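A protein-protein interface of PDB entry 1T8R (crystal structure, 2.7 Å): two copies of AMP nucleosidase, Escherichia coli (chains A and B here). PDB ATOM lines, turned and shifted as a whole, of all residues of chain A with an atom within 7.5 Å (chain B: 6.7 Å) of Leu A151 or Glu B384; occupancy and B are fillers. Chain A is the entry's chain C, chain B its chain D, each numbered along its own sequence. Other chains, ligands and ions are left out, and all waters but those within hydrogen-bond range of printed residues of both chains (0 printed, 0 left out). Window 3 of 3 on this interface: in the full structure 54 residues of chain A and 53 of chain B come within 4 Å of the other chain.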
ATOM      1  N   THR A 148      -8.972 -32.702   8.037  1.00  0.00           N
ATOM      2  CA  THR A 148      -9.373 -32.219   9.351  1.00  0.00           C
ATOM      3  C   THR A 148     -10.765 -32.752   9.644  1.00  0.00           C
ATOM      4  O   THR A 148     -11.390 -33.359   8.785  1.00  0.00           O
ATOM      5  CB  THR A 148      -9.428 -30.682   9.411  1.00  0.00           C
ATOM      6  OG1 THR A 148     -10.062 -30.180   8.229  1.00  0.00           O
ATOM      7  CG2 THR A 148      -8.036 -30.108   9.546  1.00  0.00           C
ATOM      8  N   THR A 149     -11.236 -32.537  10.866  1.00  0.00           N
ATOM      9  CA  THR A 149     -12.571 -32.979  11.255  1.00  0.00           C
ATOM     10  C   THR A 149     -13.590 -32.111  10.541  1.00  0.00           C
ATOM     11  O   THR A 149     -13.365 -30.921  10.325  1.00  0.00           O
ATOM     12  CB  THR A 149     -12.796 -32.842  12.770  1.00  0.00           C
ATOM     13  OG1 THR A 149     -12.290 -31.572  13.214  1.00  0.00           O
ATOM     14  CG2 THR A 149     -12.100 -33.971  13.517  1.00  0.00           C
ATOM     15  N   GLU A 150     -14.706 -32.716  10.163  1.00  0.00           N
ATOM     16  CA  GLU A 150     -15.763 -31.997   9.471  1.00  0.00           C
ATOM     17  C   GLU A 150     -17.037 -32.122  10.303  1.00  0.00           C
ATOM     18  O   GLU A 150     -17.782 -33.099  10.185  1.00  0.00           O
ATOM     19  CB  GLU A 150     -15.974 -32.588   8.072  1.00  0.00           C
ATOM     20  CG  GLU A 150     -14.688 -32.753   7.249  1.00  0.00           C
ATOM     21  CD  GLU A 150     -13.917 -31.445   7.058  1.00  0.00           C
ATOM     22  OE1 GLU A 150     -12.847 -31.466   6.400  1.00  0.00           O
ATOM     23  OE2 GLU A 150     -14.376 -30.397   7.563  1.00  0.00           O
ATOM     24  N   LEU A 151     -17.267 -31.125  11.151  1.00  0.00           N
ATOM     25  CA  LEU A 151     -18.419 -31.095  12.037  1.00  0.00           C
ATOM     26  C   LEU A 151     -19.713 -31.565  11.389  1.00  0.00           C
ATOM     27  O   LEU A 151     -20.542 -32.200  12.045  1.00  0.00           O
ATOM     28  CB  LEU A 151     -18.590 -29.687  12.597  1.00  0.00           C
ATOM     29  CG  LEU A 151     -18.480 -29.573  14.121  1.00  0.00           C
ATOM     30  CD1 LEU A 151     -17.291 -30.369  14.657  1.00  0.00           C
ATOM     31  CD2 LEU A 151     -18.355 -28.109  14.486  1.00  0.00           C
ATOM     32  N   ALA A 152     -19.885 -31.257  10.105  1.00  0.00           N
ATOM     33  CA  ALA A 152     -21.081 -31.666   9.372  1.00  0.00           C
ATOM     34  C   ALA A 152     -21.102 -33.188   9.198  1.00  0.00           C
ATOM     35  O   ALA A 152     -20.226 -33.766   8.543  1.00  0.00           O
ATOM     36  CB  ALA A 152     -21.128 -30.974   8.005  1.00  0.00           C
ATOM     37  N   GLN A 153     -22.101 -33.830   9.800  1.00  0.00           N
ATOM     38  CA  GLN A 153     -22.256 -35.280   9.725  1.00  0.00           C
ATOM     39  C   GLN A 153     -23.513 -35.752  10.461  1.00  0.00           C
ATOM     40  O   GLN A 153     -24.609 -35.792   9.890  1.00  0.00           O
ATOM     41  CB  GLN A 153     -21.011 -35.980  10.296  1.00  0.00           C
ATOM     42  CG  GLN A 153     -20.607 -35.556  11.711  1.00  0.00           C
ATOM     43  CD  GLN A 153     -21.288 -36.367  12.805  1.00  0.00           C
ATOM     44  OE1 GLN A 153     -22.505 -36.289  12.996  1.00  0.00           O
ATOM     45  NE2 GLN A 153     -20.496 -37.153  13.530  1.00  0.00           N
ATOM     46  N   PHE A 181     -13.439 -39.657  17.281  1.00  0.00           N
ATOM     47  CA  PHE A 181     -13.809 -38.448  17.994  1.00  0.00           C
ATOM     48  C   PHE A 181     -14.027 -38.744  19.477  1.00  0.00           C
ATOM     49  O   PHE A 181     -13.506 -38.048  20.347  1.00  0.00           O
ATOM     50  CB  PHE A 181     -15.090 -37.881  17.384  1.00  0.00           C
ATOM     51  CG  PHE A 181     -15.646 -36.692  18.109  1.00  0.00           C
ATOM     52  CD1 PHE A 181     -15.101 -35.428  17.935  1.00  0.00           C
ATOM     53  CD2 PHE A 181     -16.739 -36.829  18.957  1.00  0.00           C
ATOM     54  CE1 PHE A 181     -15.638 -34.322  18.590  1.00  0.00           C
ATOM     55  CE2 PHE A 181     -17.282 -35.715  19.620  1.00  0.00           C
ATOM     56  CZ  PHE A 181     -16.730 -34.472  19.432  1.00  0.00           C
ATOM     57  N   ARG A 185     -11.753 -38.164  23.273  1.00  0.00           N
ATOM     58  CA  ARG A 185     -12.437 -37.542  24.386  1.00  0.00           C
ATOM     59  C   ARG A 185     -12.430 -38.386  25.645  1.00  0.00           C
ATOM     60  O   ARG A 185     -12.205 -37.878  26.743  1.00  0.00           O
ATOM     61  CB  ARG A 185     -13.870 -37.260  24.001  1.00  0.00           C
ATOM     62  CG  ARG A 185     -14.171 -35.824  23.805  1.00  0.00           C
ATOM     63  CD  ARG A 185     -13.701 -35.305  22.483  1.00  0.00           C
ATOM     64  NE  ARG A 185     -14.301 -33.994  22.267  1.00  0.00           N
ATOM     65  CZ  ARG A 185     -14.045 -33.204  21.232  1.00  0.00           C
ATOM     66  NH1 ARG A 185     -13.178 -33.601  20.292  1.00  0.00           N
ATOM     67  NH2 ARG A 185     -14.659 -32.022  21.147  1.00  0.00           N
ATOM     68  N   ASP B 380     -25.046 -28.394  26.269  1.00  0.00           N
ATOM     69  CA  ASP B 380     -24.611 -29.560  25.532  1.00  0.00           C
ATOM     70  C   ASP B 380     -23.157 -29.450  25.100  1.00  0.00           C
ATOM     71  O   ASP B 380     -22.850 -28.818  24.102  1.00  0.00           O
ATOM     72  CB  ASP B 380     -25.501 -29.733  24.311  1.00  0.00           C
ATOM     73  CG  ASP B 380     -25.217 -31.002  23.562  1.00  0.00           C
ATOM     74  OD1 ASP B 380     -24.364 -31.786  24.016  1.00  0.00           O
ATOM     75  OD2 ASP B 380     -25.856 -31.217  22.513  1.00  0.00           O
ATOM     76  N   ARG B 381     -22.253 -30.067  25.839  1.00  0.00           N
ATOM     77  CA  ARG B 381     -20.861 -29.993  25.456  1.00  0.00           C
ATOM     78  C   ARG B 381     -20.562 -30.554  24.062  1.00  0.00           C
ATOM     79  O   ARG B 381     -19.687 -30.041  23.359  1.00  0.00           O
ATOM     80  CB  ARG B 381     -19.981 -30.709  26.461  1.00  0.00           C
ATOM     81  CG  ARG B 381     -18.576 -30.859  25.921  1.00  0.00           C
ATOM     82  CD  ARG B 381     -17.549 -30.202  26.824  1.00  0.00           C
ATOM     83  NE  ARG B 381     -17.539 -30.824  28.146  1.00  0.00           N
ATOM     84  CZ  ARG B 381     -16.658 -30.537  29.099  1.00  0.00           C
ATOM     85  NH1 ARG B 381     -15.708 -29.627  28.873  1.00  0.00           N
ATOM     86  NH2 ARG B 381     -16.729 -31.166  30.272  1.00  0.00           N
ATOM     87  N   ASN B 382     -21.267 -31.610  23.669  1.00  0.00           N
ATOM     88  CA  ASN B 382     -21.036 -32.198  22.361  1.00  0.00           C
ATOM     89  C   ASN B 382     -21.984 -31.632  21.330  1.00  0.00           C
ATOM     90  O   ASN B 382     -22.459 -32.353  20.464  1.00  0.00           O
ATOM     91  CB  ASN B 382     -21.180 -33.713  22.417  1.00  0.00           C
ATOM     92  CG  ASN B 382     -20.105 -34.363  23.256  1.00  0.00           C
ATOM     93  OD1 ASN B 382     -18.937 -34.031  23.121  1.00  0.00           O
ATOM     94  ND2 ASN B 382     -20.489 -35.300  24.123  1.00  0.00           N
ATOM     95  N   TRP B 383     -22.243 -30.332  21.416  1.00  0.00           N
ATOM     96  CA  TRP B 383     -23.149 -29.675  20.481  1.00  0.00           C
ATOM     97  C   TRP B 383     -22.699 -29.891  19.039  1.00  0.00           C
ATOM     98  O   TRP B 383     -23.518 -29.874  18.125  1.00  0.00           O
ATOM     99  CB  TRP B 383     -23.258 -28.168  20.787  1.00  0.00           C
ATOM    100  CG  TRP B 383     -21.963 -27.440  20.672  1.00  0.00           C
ATOM    101  CD1 TRP B 383     -21.032 -27.279  21.645  1.00  0.00           C
ATOM    102  CD2 TRP B 383     -21.399 -26.882  19.481  1.00  0.00           C
ATOM    103  NE1 TRP B 383     -19.917 -26.663  21.136  1.00  0.00           N
ATOM    104  CE2 TRP B 383     -20.119 -26.410  19.810  1.00  0.00           C
ATOM    105  CE3 TRP B 383     -21.855 -26.741  18.170  1.00  0.00           C
ATOM    106  CZ2 TRP B 383     -19.287 -25.811  18.880  1.00  0.00           C
ATOM    107  CZ3 TRP B 383     -21.038 -26.148  17.242  1.00  0.00           C
ATOM    108  CH2 TRP B 383     -19.760 -25.687  17.599  1.00  0.00           C
ATOM    109  N   GLU B 384     -21.401 -30.101  18.837  1.00  0.00           N
ATOM    110  CA  GLU B 384     -20.862 -30.333  17.498  1.00  0.00           C
ATOM    111  C   GLU B 384     -21.513 -31.534  16.804  1.00  0.00           C
ATOM    112  O   GLU B 384     -21.564 -31.581  15.576  1.00  0.00           O
ATOM    113  CB  GLU B 384     -19.342 -30.565  17.546  1.00  0.00           C
ATOM    114  CG  GLU B 384     -18.540 -29.457  18.211  1.00  0.00           C
ATOM    115  CD  GLU B 384     -18.301 -29.711  19.697  1.00  0.00           C
ATOM    116  OE1 GLU B 384     -19.217 -30.242  20.358  1.00  0.00           O
ATOM    117  OE2 GLU B 384     -17.206 -29.369  20.207  1.00  0.00           O
ATOM    118  N   LEU B 385     -21.993 -32.508  17.574  1.00  0.00           N
ATOM    119  CA  LEU B 385     -22.623 -33.679  16.980  1.00  0.00           C
ATOM    120  C   LEU B 385     -23.993 -33.342  16.404  1.00  0.00           C
ATOM    121  O   LEU B 385     -24.629 -34.188  15.779  1.00  0.00           O
ATOM    122  CB  LEU B 385     -22.762 -34.801  18.009  1.00  0.00           C
ATOM    123  CG  LEU B 385     -21.467 -35.336  18.637  1.00  0.00           C
ATOM    124  CD1 LEU B 385     -21.815 -36.313  19.744  1.00  0.00           C
ATOM    125  CD2 LEU B 385     -20.591 -36.016  17.598  1.00  0.00           C
ATOM    126  N   ARG B 386     -24.450 -32.111  16.620  1.00  0.00           N
ATOM    127  CA  ARG B 386     -25.743 -31.666  16.099  1.00  0.00           C
ATOM    128  C   ARG B 386     -25.635 -30.291  15.460  1.00  0.00           C
ATOM    129  O   ARG B 386     -26.595 -29.523  15.488  1.00  0.00           O
ATOM    130  CB  ARG B 386     -26.785 -31.559  17.205  1.00  0.00           C
ATOM    131  CG  ARG B 386     -26.994 -32.785  18.024  1.00  0.00           C
ATOM    132  CD  ARG B 386     -28.134 -32.543  18.987  1.00  0.00           C
ATOM    133  NE  ARG B 386     -29.371 -32.318  18.253  1.00  0.00           N
ATOM    134  CZ  ARG B 386     -30.154 -31.254  18.406  1.00  0.00           C
ATOM    135  NH1 ARG B 386     -29.827 -30.306  19.279  1.00  0.00           N
ATOM    136  NH2 ARG B 386     -31.256 -31.139  17.667  1.00  0.00           N
ATOM    137  N   TYR B 387     -24.483 -29.976  14.887  1.00  0.00           N
ATOM    138  CA  TYR B 387     -24.308 -28.672  14.279  1.00  0.00           C
ATOM    139  C   TYR B 387     -25.444 -28.248  13.362  1.00  0.00           C
ATOM    140  O   TYR B 387     -25.989 -27.170  13.528  1.00  0.00           O
ATOM    141  CB  TYR B 387     -22.989 -28.590  13.508  1.00  0.00           C
ATOM    142  CG  TYR B 387     -22.792 -27.234  12.866  1.00  0.00           C
ATOM    143  CD1 TYR B 387     -22.942 -26.065  13.615  1.00  0.00           C
ATOM    144  CD2 TYR B 387     -22.508 -27.116  11.504  1.00  0.00           C
ATOM    145  CE1 TYR B 387     -22.823 -24.816  13.032  1.00  0.00           C
ATOM    146  CE2 TYR B 387     -22.385 -25.861  10.902  1.00  0.00           C
ATOM    147  CZ  TYR B 387     -22.547 -24.716  11.672  1.00  0.00           C
ATOM    148  OH  TYR B 387     -22.443 -23.472  11.079  1.00  0.00           O
ATOM    149  N   SER B 388     -25.789 -29.083  12.396  1.00  0.00           N
ATOM    150  CA  SER B 388     -26.858 -28.757  11.465  1.00  0.00           C
ATOM    151  C   SER B 388     -28.104 -28.227  12.171  1.00  0.00           C
ATOM    152  O   SER B 388     -28.688 -27.230  11.746  1.00  0.00           O
ATOM    153  CB  SER B 388     -27.215 -29.991  10.646  1.00  0.00           C
ATOM    154  OG  SER B 388     -27.479 -31.097  11.502  1.00  0.00           O
ATOM    155  N   ASP B 428     -10.393 -22.483  20.739  1.00  0.00           N
ATOM    156  CA  ASP B 428     -10.459 -23.355  19.585  1.00  0.00           C
ATOM    157  C   ASP B 428     -11.495 -22.927  18.566  1.00  0.00           C
ATOM    158  O   ASP B 428     -12.288 -22.030  18.817  1.00  0.00           O
ATOM    159  CB  ASP B 428     -10.700 -24.799  20.013  1.00  0.00           C
ATOM    160  CG  ASP B 428     -12.088 -25.026  20.519  1.00  0.00           C
ATOM    161  OD1 ASP B 428     -12.454 -24.406  21.547  1.00  0.00           O
ATOM    162  OD2 ASP B 428     -12.818 -25.827  19.889  1.00  0.00           O
ATOM    163  N   LYS B 429     -11.459 -23.565  17.403  1.00  0.00           N
ATOM    164  CA  LYS B 429     -12.381 -23.256  16.324  1.00  0.00           C
ATOM    165  C   LYS B 429     -13.010 -24.532  15.774  1.00  0.00           C
ATOM    166  O   LYS B 429     -12.518 -25.098  14.804  1.00  0.00           O
ATOM    167  CB  LYS B 429     -11.632 -22.517  15.228  1.00  0.00           C
ATOM    168  CG  LYS B 429     -10.948 -21.261  15.738  1.00  0.00           C
ATOM    169  CD  LYS B 429     -10.242 -20.499  14.616  1.00  0.00           C
ATOM    170  CE  LYS B 429     -11.221 -19.963  13.558  1.00  0.00           C
ATOM    171  NZ  LYS B 429     -12.277 -19.154  14.214  1.00  0.00           N
ATOM    172  N   PRO B 430     -14.115 -24.987  16.395  1.00  0.00           N
ATOM    173  CA  PRO B 430     -14.883 -26.187  16.053  1.00  0.00           C
ATOM    174  C   PRO B 430     -15.334 -26.257  14.602  1.00  0.00           C
ATOM    175  O   PRO B 430     -15.276 -27.314  13.980  1.00  0.00           O
ATOM    176  CB  PRO B 430     -16.077 -26.114  17.000  1.00  0.00           C
ATOM    177  CG  PRO B 430     -15.561 -25.329  18.144  1.00  0.00           C
ATOM    178  CD  PRO B 430     -14.784 -24.249  17.477  1.00  0.00           C
ATOM    179  N   LEU B 431     -15.787 -25.130  14.069  1.00  0.00           N
ATOM    180  CA  LEU B 431     -16.282 -25.076  12.698  1.00  0.00           C
ATOM    181  C   LEU B 431     -15.202 -24.953  11.642  1.00  0.00           C
ATOM    182  O   LEU B 431     -15.499 -24.898  10.456  1.00  0.00           O
ATOM    183  CB  LEU B 431     -17.255 -23.904  12.544  1.00  0.00           C
ATOM    184  CG  LEU B 431     -18.734 -24.104  12.898  1.00  0.00           C
ATOM    185  CD1 LEU B 431     -18.902 -25.074  14.064  1.00  0.00           C
ATOM    186  CD2 LEU B 431     -19.333 -22.734  13.198  1.00  0.00           C
ATOM    187  N   HIS B 432     -13.948 -24.915  12.070  1.00  0.00           N
ATOM    188  CA  HIS B 432     -12.862 -24.759  11.126  1.00  0.00           C
ATOM    189  C   HIS B 432     -11.676 -25.689  11.311  1.00  0.00           C
ATOM    190  O   HIS B 432     -10.525 -25.257  11.247  1.00  0.00           O
ATOM    191  CB  HIS B 432     -12.399 -23.309  11.127  1.00  0.00           C
ATOM    192  CG  HIS B 432     -13.490 -22.336  10.803  1.00  0.00           C
ATOM    193  ND1 HIS B 432     -14.392 -21.886  11.742  1.00  0.00           N
ATOM    194  CD2 HIS B 432     -13.859 -21.773   9.629  1.00  0.00           C
ATOM    195  CE1 HIS B 432     -15.271 -21.090  11.161  1.00  0.00           C
ATOM    196  NE2 HIS B 432     -14.971 -21.007   9.878  1.00  0.00           N
ATOM    197  N   ILE B 435     -10.496 -28.418  16.446  1.00  0.00           N
ATOM    198  CA  ILE B 435     -11.136 -28.745  17.701  1.00  0.00           C
ATOM    199  C   ILE B 435     -10.025 -29.111  18.702  1.00  0.00           C
ATOM    200  O   ILE B 435      -9.242 -30.041  18.475  1.00  0.00           O
ATOM    201  CB  ILE B 435     -12.138 -29.906  17.522  1.00  0.00           C
ATOM    202  CG1 ILE B 435     -13.169 -29.527  16.451  1.00  0.00           C
ATOM    203  CG2 ILE B 435     -12.852 -30.185  18.838  1.00  0.00           C
ATOM    204  CD1 ILE B 435     -14.255 -30.556  16.227  1.00  0.00           C
ATOM    205  N   LEU B 437      -9.200 -29.305  23.146  1.00  0.00           N
ATOM    206  CA  LEU B 437      -9.874 -29.416  24.437  1.00  0.00           C
ATOM    207  C   LEU B 437      -9.049 -28.834  25.580  1.00  0.00           C
ATOM    208  O   LEU B 437      -7.818 -28.874  25.553  1.00  0.00           O
ATOM    209  CB  LEU B 437     -10.219 -30.880  24.742  1.00  0.00           C
ATOM    210  CG  LEU B 437     -11.156 -31.613  23.769  1.00  0.00           C
ATOM    211  CD1 LEU B 437     -11.722 -32.848  24.471  1.00  0.00           C
ATOM    212  CD2 LEU B 437     -12.300 -30.697  23.316  1.00  0.00           C
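Of the printed residues of chain B, Thr A149 touches Ile B435. Leu A151 touches just these residues of chain B: Glu B384, Pro B430, Leu B431 and Ile B435. Of the printed residues of chain B, Arg A185 touches Glu B384, Ile B435 and Leu B437. Of chain A, only Leu A151 and Arg A185 come within 4 Å of Glu B384. Ser B388 touches none of the printed residues of chain A. Lys B429 touches none of the printed residues of chain A. The nearest printed residue of chain B that does not touch Arg A185 is Asn B382 (4.7 Å).
No position is printed for both chains. Of the 9 pairs that touch across the chains among the printed residues, none has its exchanged pair printed and touching as well.
Among the printed residues, merely in contact across the chains: Thr A149 with Ile B435 (3.7 Å), Leu A151 with Glu B384 (3.5 Å), Leu A151 with Pro B430 (3.2 Å), Leu A151 with Leu B431 (3.1 Å), Leu A151 with Ile B435 (3.4 Å), Phe A181 with Leu B385 (3.9 Å), Arg A185 with Ile B435 (3.5 Å) and Arg A185 with Leu B437 (3.5 Å).
NH2 of Arg A185 lies within salt-bridge range of OE2 of Glu B384 (3.8 Å).
Of the 8 printed residues of chain A, 4 touch a printed residue of chain B. Printed residues of chain A that touch a printed residue of chain B: Thr A149, Leu A151, Phe A181 and Arg A185. Printed residues of chain B that touch a printed residue of chain A: Glu B384, Leu B385, Pro B430, Leu B431, Ile B435 and Leu B437. Hydrophobic or aromatic side chains of chain B that line the printed part of chain A: Leu B385, Pro B430, Leu B431, Ile B435 and Leu B437.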
